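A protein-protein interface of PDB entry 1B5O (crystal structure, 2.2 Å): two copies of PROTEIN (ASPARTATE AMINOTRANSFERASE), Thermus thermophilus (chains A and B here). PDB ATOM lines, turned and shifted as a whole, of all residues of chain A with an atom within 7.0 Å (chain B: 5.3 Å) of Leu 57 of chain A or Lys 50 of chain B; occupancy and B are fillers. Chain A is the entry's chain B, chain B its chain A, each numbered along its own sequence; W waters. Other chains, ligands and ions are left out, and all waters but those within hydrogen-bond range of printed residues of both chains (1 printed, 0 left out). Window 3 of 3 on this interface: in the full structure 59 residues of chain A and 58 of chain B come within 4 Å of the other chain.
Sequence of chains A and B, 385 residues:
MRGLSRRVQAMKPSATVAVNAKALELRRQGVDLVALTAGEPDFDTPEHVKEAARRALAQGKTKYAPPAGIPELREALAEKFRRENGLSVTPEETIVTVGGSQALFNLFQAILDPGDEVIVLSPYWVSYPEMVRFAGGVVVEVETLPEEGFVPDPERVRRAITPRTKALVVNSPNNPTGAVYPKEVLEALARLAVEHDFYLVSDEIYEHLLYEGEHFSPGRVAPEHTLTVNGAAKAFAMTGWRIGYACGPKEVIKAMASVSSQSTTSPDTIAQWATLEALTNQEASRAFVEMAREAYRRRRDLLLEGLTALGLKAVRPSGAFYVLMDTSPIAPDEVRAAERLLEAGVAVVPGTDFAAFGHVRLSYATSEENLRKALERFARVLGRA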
ATOM      1  N   GLU A  51      14.139  12.089 -14.311  1.00  0.00           N
ATOM      2  CA  GLU A  51      15.228  11.925 -15.267  1.00  0.00           C
ATOM      3  C   GLU A  51      15.954  10.597 -15.072  1.00  0.00           C
ATOM      4  O   GLU A  51      16.308   9.924 -16.042  1.00  0.00           O
ATOM      5  CB  GLU A  51      16.216  13.092 -15.141  1.00  0.00           C
ATOM      6  CG  GLU A  51      17.073  13.307 -16.369  1.00  0.00           C
ATOM      7  CD  GLU A  51      16.256  13.345 -17.659  1.00  0.00           C
ATOM      8  OE1 GLU A  51      15.286  14.131 -17.755  1.00  0.00           O
ATOM      9  OE2 GLU A  51      16.589  12.575 -18.579  1.00  0.00           O
ATOM     10  N   ALA A  52      16.158  10.215 -13.815  1.00  0.00           N
ATOM     11  CA  ALA A  52      16.821   8.957 -13.506  1.00  0.00           C
ATOM     12  C   ALA A  52      15.958   7.802 -13.995  1.00  0.00           C
ATOM     13  O   ALA A  52      16.469   6.766 -14.395  1.00  0.00           O
ATOM     14  CB  ALA A  52      17.060   8.842 -12.017  1.00  0.00           C
ATOM     15  N   ALA A  53      14.644   7.985 -13.945  1.00  0.00           N
ATOM     16  CA  ALA A  53      13.704   6.965 -14.406  1.00  0.00           C
ATOM     17  C   ALA A  53      13.855   6.785 -15.915  1.00  0.00           C
ATOM     18  O   ALA A  53      13.902   5.660 -16.414  1.00  0.00           O
ATOM     19  CB  ALA A  53      12.272   7.371 -14.060  1.00  0.00           C
ATOM     20  N   ARG A  54      13.915   7.906 -16.630  1.00  0.00           N
ATOM     21  CA  ARG A  54      14.086   7.903 -18.079  1.00  0.00           C
ATOM     22  C   ARG A  54      15.386   7.202 -18.491  1.00  0.00           C
ATOM     23  O   ARG A  54      15.401   6.454 -19.462  1.00  0.00           O
ATOM     24  CB  ARG A  54      14.073   9.333 -18.610  1.00  0.00           C
ATOM     25  CG  ARG A  54      12.732  10.007 -18.481  1.00  0.00           C
ATOM     26  CD  ARG A  54      12.831  11.499 -18.751  1.00  0.00           C
ATOM     27  NE  ARG A  54      11.544  12.139 -18.516  1.00  0.00           N
ATOM     28  CZ  ARG A  54      11.356  13.207 -17.750  1.00  0.00           C
ATOM     29  NH1 ARG A  54      12.377  13.791 -17.136  1.00  0.00           N
ATOM     30  NH2 ARG A  54      10.123  13.643 -17.548  1.00  0.00           N
ATOM     31  N   ARG A  55      16.468   7.440 -17.747  1.00  0.00           N
ATOM     32  CA  ARG A  55      17.752   6.808 -18.035  1.00  0.00           C
ATOM     33  C   ARG A  55      17.677   5.295 -17.860  1.00  0.00           C
ATOM     34  O   ARG A  55      18.195   4.545 -18.687  1.00  0.00           O
ATOM     35  CB  ARG A  55      18.869   7.375 -17.145  1.00  0.00           C
ATOM     36  CG  ARG A  55      19.372   8.746 -17.571  1.00  0.00           C
ATOM     37  CD  ARG A  55      20.687   9.125 -16.885  1.00  0.00           C
ATOM     38  NE  ARG A  55      20.571   9.286 -15.437  1.00  0.00           N
ATOM     39  CZ  ARG A  55      20.178  10.403 -14.826  1.00  0.00           C
ATOM     40  NH1 ARG A  55      19.851  11.484 -15.527  1.00  0.00           N
ATOM     41  NH2 ARG A  55      20.125  10.445 -13.502  1.00  0.00           N
ATOM     42  N   ALA A  56      17.025   4.851 -16.785  1.00  0.00           N
ATOM     43  CA  ALA A  56      16.882   3.425 -16.514  1.00  0.00           C
ATOM     44  C   ALA A  56      16.127   2.750 -17.661  1.00  0.00           C
ATOM     45  O   ALA A  56      16.503   1.663 -18.103  1.00  0.00           O
ATOM     46  CB  ALA A  56      16.158   3.204 -15.182  1.00  0.00           C
ATOM     47  N   LEU A  57      15.093   3.420 -18.164  1.00  0.00           N
ATOM     48  CA  LEU A  57      14.292   2.905 -19.270  1.00  0.00           C
ATOM     49  C   LEU A  57      15.145   2.698 -20.514  1.00  0.00           C
ATOM     50  O   LEU A  57      15.077   1.651 -21.160  1.00  0.00           O
ATOM     51  CB  LEU A  57      13.153   3.875 -19.603  1.00  0.00           C
ATOM     52  CG  LEU A  57      11.858   3.837 -18.787  1.00  0.00           C
ATOM     53  CD1 LEU A  57      10.902   4.917 -19.287  1.00  0.00           C
ATOM     54  CD2 LEU A  57      11.212   2.465 -18.905  1.00  0.00           C
ATOM     55  N   ALA A  58      15.943   3.706 -20.843  1.00  0.00           N
ATOM     56  CA  ALA A  58      16.815   3.657 -22.008  1.00  0.00           C
ATOM     57  C   ALA A  58      17.979   2.684 -21.824  1.00  0.00           C
ATOM     58  O   ALA A  58      18.524   2.170 -22.796  1.00  0.00           O
ATOM     59  CB  ALA A  58      17.331   5.047 -22.322  1.00  0.00           C
ATOM     60  N   GLN A  59      18.373   2.447 -20.579  1.00  0.00           N
ATOM     61  CA  GLN A  59      19.457   1.521 -20.302  1.00  0.00           C
ATOM     62  C   GLN A  59      18.916   0.097 -20.211  1.00  0.00           C
ATOM     63  O   GLN A  59      19.650  -0.841 -19.908  1.00  0.00           O
ATOM     64  CB  GLN A  59      20.179   1.909 -19.012  1.00  0.00           C
ATOM     65  CG  GLN A  59      20.981   3.208 -19.115  1.00  0.00           C
ATOM     66  CD  GLN A  59      21.696   3.580 -17.817  1.00  0.00           C
ATOM     67  OE1 GLN A  59      22.100   4.724 -17.624  1.00  0.00           O
ATOM     68  NE2 GLN A  59      21.879   2.607 -16.937  1.00  0.00           N
ATOM     69  N   GLY A  60      17.618  -0.053 -20.450  1.00  0.00           N
ATOM     70  CA  GLY A  60      17.008  -1.368 -20.414  1.00  0.00           C
ATOM     71  C   GLY A  60      17.018  -2.083 -19.080  1.00  0.00           C
ATOM     72  O   GLY A  60      17.125  -3.305 -19.041  1.00  0.00           O
ATOM     73  N   LYS A  61      16.934  -1.333 -17.987  1.00  0.00           N
ATOM     74  CA  LYS A  61      16.901  -1.926 -16.650  1.00  0.00           C
ATOM     75  C   LYS A  61      15.442  -2.280 -16.366  1.00  0.00           C
ATOM     76  O   LYS A  61      14.779  -1.661 -15.527  1.00  0.00           O
ATOM     77  CB  LYS A  61      17.456  -0.935 -15.633  1.00  0.00           C
ATOM     78  CG  LYS A  61      18.932  -0.682 -15.845  1.00  0.00           C
ATOM     79  CD  LYS A  61      19.470   0.432 -14.979  1.00  0.00           C
ATOM     80  CE  LYS A  61      20.988   0.326 -14.882  1.00  0.00           C
ATOM     81  NZ  LYS A  61      21.601   1.426 -14.078  1.00  0.00           N
ATOM     82  N   THR A  62      14.974  -3.316 -17.060  1.00  0.00           N
ATOM     83  CA  THR A  62      13.590  -3.757 -16.985  1.00  0.00           C
ATOM     84  C   THR A  62      13.399  -5.230 -16.610  1.00  0.00           C
ATOM     85  O   THR A  62      12.346  -5.807 -16.872  1.00  0.00           O
ATOM     86  CB  THR A  62      12.921  -3.501 -18.350  1.00  0.00           C
ATOM     87  OG1 THR A  62      13.620  -4.242 -19.357  1.00  0.00           O
ATOM     88  CG2 THR A  62      12.994  -2.021 -18.717  1.00  0.00           C
ATOM     89  N   ILE A 270      12.424  -0.029 -12.422  1.00  0.00           N
ATOM     90  CA  ILE A 270      12.601   1.362 -12.843  1.00  0.00           C
ATOM     91  C   ILE A 270      12.452   2.315 -11.641  1.00  0.00           C
ATOM     92  O   ILE A 270      13.178   3.299 -11.520  1.00  0.00           O
ATOM     93  CB  ILE A 270      11.569   1.767 -13.940  1.00  0.00           C
ATOM     94  CG1 ILE A 270      11.828   1.008 -15.246  1.00  0.00           C
ATOM     95  CG2 ILE A 270      11.616   3.264 -14.196  1.00  0.00           C
ATOM     96  CD1 ILE A 270      11.233  -0.385 -15.286  1.00  0.00           C
ATOM     97  N   ASP B  44      14.393  -6.853 -24.506  1.00  0.00           N
ATOM     98  CA  ASP B  44      14.073  -5.709 -23.661  1.00  0.00           C
ATOM     99  C   ASP B  44      12.610  -5.408 -23.993  1.00  0.00           C
ATOM    100  O   ASP B  44      12.092  -5.902 -24.993  1.00  0.00           O
ATOM    101  CB  ASP B  44      14.963  -4.517 -24.033  1.00  0.00           C
ATOM    102  CG  ASP B  44      14.944  -3.400 -22.986  1.00  0.00           C
ATOM    103  OD1 ASP B  44      14.229  -3.497 -21.965  1.00  0.00           O
ATOM    104  OD2 ASP B  44      15.661  -2.404 -23.190  1.00  0.00           O
ATOM    105  N   THR B  45      11.927  -4.637 -23.156  1.00  0.00           N
ATOM    106  CA  THR B  45      10.530  -4.324 -23.436  1.00  0.00           C
ATOM    107  C   THR B  45      10.430  -3.405 -24.663  1.00  0.00           C
ATOM    108  O   THR B  45      11.294  -2.551 -24.873  1.00  0.00           O
ATOM    109  CB  THR B  45       9.771  -3.764 -22.173  1.00  0.00           C
ATOM    110  OG1 THR B  45       9.023  -2.583 -22.503  1.00  0.00           O
ATOM    111  CG2 THR B  45      10.716  -3.487 -21.034  1.00  0.00           C
ATOM    112  N   PRO B  46       9.426  -3.639 -25.536  1.00  0.00           N
ATOM    113  CA  PRO B  46       9.218  -2.836 -26.749  1.00  0.00           C
ATOM    114  C   PRO B  46       9.117  -1.329 -26.511  1.00  0.00           C
ATOM    115  O   PRO B  46       8.648  -0.880 -25.463  1.00  0.00           O
ATOM    116  CB  PRO B  46       7.934  -3.426 -27.348  1.00  0.00           C
ATOM    117  CG  PRO B  46       7.263  -4.112 -26.193  1.00  0.00           C
ATOM    118  CD  PRO B  46       8.419  -4.712 -25.445  1.00  0.00           C
ATOM    119  N   GLU B  47       9.569  -0.561 -27.502  1.00  0.00           N
ATOM    120  CA  GLU B  47       9.579   0.895 -27.439  1.00  0.00           C
ATOM    121  C   GLU B  47       8.263   1.615 -27.209  1.00  0.00           C
ATOM    122  O   GLU B  47       8.252   2.674 -26.584  1.00  0.00           O
ATOM    123  CB  GLU B  47      10.274   1.482 -28.668  1.00  0.00           C
ATOM    124  CG  GLU B  47      11.751   1.788 -28.451  1.00  0.00           C
ATOM    125  CD  GLU B  47      11.994   2.811 -27.346  1.00  0.00           C
ATOM    126  OE1 GLU B  47      11.342   3.882 -27.357  1.00  0.00           O
ATOM    127  OE2 GLU B  47      12.847   2.544 -26.470  1.00  0.00           O
ATOM    128  N   HIS B  48       7.162   1.077 -27.725  1.00  0.00           N
ATOM    129  CA  HIS B  48       5.875   1.729 -27.528  1.00  0.00           C
ATOM    130  C   HIS B  48       5.443   1.693 -26.060  1.00  0.00           C
ATOM    131  O   HIS B  48       4.793   2.618 -25.574  1.00  0.00           O
ATOM    132  CB  HIS B  48       4.796   1.166 -28.472  1.00  0.00           C
ATOM    133  CG  HIS B  48       4.493  -0.289 -28.284  1.00  0.00           C
ATOM    134  ND1 HIS B  48       3.244  -0.744 -27.916  1.00  0.00           N
ATOM    135  CD2 HIS B  48       5.259  -1.392 -28.451  1.00  0.00           C
ATOM    136  CE1 HIS B  48       3.254  -2.065 -27.863  1.00  0.00           C
ATOM    137  NE2 HIS B  48       4.464  -2.481 -28.183  1.00  0.00           N
ATOM    138  N   VAL B  49       5.854   0.648 -25.347  1.00  0.00           N
ATOM    139  CA  VAL B  49       5.530   0.520 -23.929  1.00  0.00           C
ATOM    140  C   VAL B  49       6.374   1.567 -23.196  1.00  0.00           C
ATOM    141  O   VAL B  49       5.859   2.353 -22.402  1.00  0.00           O
ATOM    142  CB  VAL B  49       5.848  -0.910 -23.400  1.00  0.00           C
ATOM    143  CG1 VAL B  49       5.641  -0.996 -21.889  1.00  0.00           C
ATOM    144  CG2 VAL B  49       4.973  -1.935 -24.108  1.00  0.00           C
ATOM    145  N   LYS B  50       7.660   1.608 -23.523  1.00  0.00           N
ATOM    146  CA  LYS B  50       8.568   2.565 -22.917  1.00  0.00           C
ATOM    147  C   LYS B  50       8.098   3.983 -23.185  1.00  0.00           C
ATOM    148  O   LYS B  50       8.222   4.849 -22.332  1.00  0.00           O
ATOM    149  CB  LYS B  50       9.981   2.400 -23.468  1.00  0.00           C
ATOM    150  CG  LYS B  50      10.692   1.129 -23.022  1.00  0.00           C
ATOM    151  CD  LYS B  50      12.161   1.215 -23.391  1.00  0.00           C
ATOM    152  CE  LYS B  50      12.954   0.032 -22.882  1.00  0.00           C
ATOM    153  NZ  LYS B  50      14.338   0.098 -23.442  1.00  0.00           N
ATOM    154  N   GLU B  51       7.543   4.207 -24.371  1.00  0.00           N
ATOM    155  CA  GLU B  51       7.063   5.526 -24.747  1.00  0.00           C
ATOM    156  C   GLU B  51       5.823   5.963 -23.959  1.00  0.00           C
ATOM    157  O   GLU B  51       5.667   7.145 -23.659  1.00  0.00           O
ATOM    158  CB  GLU B  51       6.802   5.585 -26.254  1.00  0.00           C
ATOM    159  CG  GLU B  51       6.307   6.937 -26.758  1.00  0.00           C
ATOM    160  CD  GLU B  51       7.245   8.091 -26.421  1.00  0.00           C
ATOM    161  OE1 GLU B  51       8.481   7.882 -26.366  1.00  0.00           O
ATOM    162  OE2 GLU B  51       6.735   9.217 -26.214  1.00  0.00           O
ATOM    163  N   ALA B  52       4.946   5.009 -23.643  1.00  0.00           N
ATOM    164  CA  ALA B  52       3.740   5.290 -22.863  1.00  0.00           C
ATOM    165  C   ALA B  52       4.159   5.678 -21.450  1.00  0.00           C
ATOM    166  O   ALA B  52       3.521   6.513 -20.819  1.00  0.00           O
ATOM    167  CB  ALA B  52       2.837   4.064 -22.818  1.00  0.00           C
ATOM    168  N   ALA B  53       5.236   5.053 -20.969  1.00  0.00           N
ATOM    169  CA  ALA B  53       5.787   5.317 -19.641  1.00  0.00           C
ATOM    170  C   ALA B  53       6.355   6.735 -19.548  1.00  0.00           C
ATOM    171  O   ALA B  53       6.160   7.417 -18.547  1.00  0.00           O
ATOM    172  CB  ALA B  53       6.870   4.297 -19.308  1.00  0.00           C
ATOM    173  N   ARG B  54       7.067   7.168 -20.585  1.00  0.00           N
ATOM    174  CA  ARG B  54       7.638   8.513 -20.604  1.00  0.00           C
ATOM    175  C   ARG B  54       6.531   9.555 -20.600  1.00  0.00           C
ATOM    176  O   ARG B  54       6.662  10.586 -19.951  1.00  0.00           O
ATOM    177  CB  ARG B  54       8.529   8.717 -21.829  1.00  0.00           C
ATOM    178  CG  ARG B  54       9.808   7.907 -21.807  1.00  0.00           C
ATOM    179  CD  ARG B  54      10.639   8.129 -23.074  1.00  0.00           C
ATOM    180  NE  ARG B  54      11.691   7.121 -23.178  1.00  0.00           N
ATOM    181  CZ  ARG B  54      11.804   6.248 -24.175  1.00  0.00           C
ATOM    182  NH1 ARG B  54      10.940   6.257 -25.184  1.00  0.00           N
ATOM    183  NH2 ARG B  54      12.741   5.306 -24.122  1.00  0.00           N
ATOM    184  N   LEU B  57       5.054  10.057 -17.143  1.00  0.00           N
ATOM    185  CA  LEU B  57       5.968  10.840 -16.313  1.00  0.00           C
ATOM    186  C   LEU B  57       5.804  12.332 -16.584  1.00  0.00           C
ATOM    187  O   LEU B  57       5.713  13.135 -15.655  1.00  0.00           O
ATOM    188  CB  LEU B  57       7.424  10.446 -16.586  1.00  0.00           C
ATOM    189  CG  LEU B  57       7.975   9.190 -15.916  1.00  0.00           C
ATOM    190  CD1 LEU B  57       9.420   8.985 -16.348  1.00  0.00           C
ATOM    191  CD2 LEU B  57       7.879   9.325 -14.400  1.00  0.00           C
ATOM    192  N   TRP B 241       8.634  -4.626 -14.490  1.00  0.00           N
ATOM    193  CA  TRP B 241       7.616  -3.600 -14.277  1.00  0.00           C
ATOM    194  C   TRP B 241       6.631  -3.987 -13.173  1.00  0.00           C
ATOM    195  O   TRP B 241       5.963  -3.126 -12.609  1.00  0.00           O
ATOM    196  CB  TRP B 241       6.857  -3.308 -15.571  1.00  0.00           C
ATOM    197  CG  TRP B 241       7.713  -2.718 -16.652  1.00  0.00           C
ATOM    198  CD1 TRP B 241       8.677  -3.358 -17.376  1.00  0.00           C
ATOM    199  CD2 TRP B 241       7.638  -1.385 -17.171  1.00  0.00           C
ATOM    200  NE1 TRP B 241       9.197  -2.512 -18.323  1.00  0.00           N
ATOM    201  CE2 TRP B 241       8.576  -1.297 -18.226  1.00  0.00           C
ATOM    202  CE3 TRP B 241       6.864  -0.259 -16.860  1.00  0.00           C
ATOM    203  CZ2 TRP B 241       8.760  -0.127 -18.969  1.00  0.00           C
ATOM    204  CZ3 TRP B 241       7.048   0.907 -17.602  1.00  0.00           C
ATOM    205  CH2 TRP B 241       7.989   0.960 -18.645  1.00  0.00           C
HETATM  206  O   HOH W   1       9.005  12.075 -19.908  1.00  0.00           O
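Leu 57 of chain A touches just these residues of chain B: Lys 50 and Trp 241.
Lys 50 of chain B touches just one residue of chain A: Leu 57 (2.9 Å).
Of the printed residues of chain B, Thr 62 of chain A touches Asp 44, Thr 45 and Trp 241.
Of the printed residues of chain A, Asp 44 of chain B touches Gly 60 (3.3 Å) and Thr 62 (2.8 Å).
Of the printed residues of chain A, Leu 57 of chain B touches Ala 53.
Printed residues of chain A within 4 Å of Trp 241 of chain B: Leu 57 (3.6 Å) and Thr 62 (3.8 Å).
Of the printed residues of chain B, Gly 60 of chain A touches Asp 44.
Ile 270 of chain A touches none of the printed residues of chain B.
Ala 52 of chain B touches none of the printed residues of chain A.
The nearest printed residue of chain B that does not touch Leu 57 of chain A is Arg 54 of chain B (4.1 Å).
The nearest printed residue of chain A that does not touch Thr 45 of chain B is Leu 57 of chain A (6.3 Å).
OD2 of Asp 44 of chain B is in salt-bridge range of NZ of Lys 50 of chain B, 2.8 Å away.
Ala 53 of chain A touches Leu 57 of chain B, but with the chains exchanged Leu 57 of chain A does not touch Ala 53 of chain B (4.1 Å).
Positions printed for both chains: 51, 52, 53, 54 and 57.
The side-chain carboxylate (OD1) of Asp 44 of chain B lies within hydrogen-bond range of the side-chain hydroxyl (OG1) of Thr 62 of chain A.
O of Leu 57 of chain A sits at hydrogen-bond distance from NZ of Lys 50 of chain B (2.9 Å).
Water W1 bridges O of Arg 54 of chain B (2.8 Å) and NE of Arg 54 of chain A (2.9 Å).
Ala 53 of chain A touches Leu 57 of chain B (CB to CD1, 3.997 Å).
CD2 of Leu 57 of chain A touches CH2 of Trp 241 of chain B (3.6 Å).
Gly 60 of chain A touches Asp 44 of chain B (CA to OD2, 3.3 Å).
Thr 45 of chain B touches Thr 62 of chain A.
NE1 of Trp 241 of chain B touches CG2 of Thr 62 of chain A, 3.8 Å away.
Of the 13 printed residues of chain A, 4 touch a printed residue of chain B.
Hydrophobic or aromatic side chains of chain A within 4 Å of the printed part of chain B: Ala 53 and Leu 57.
Of the 13 printed residues of chain B, 5 touch a printed residue of chain A.
Hydrophobic or aromatic side chains of chain B that line the printed part of chain A: Leu 57 and Trp 241.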
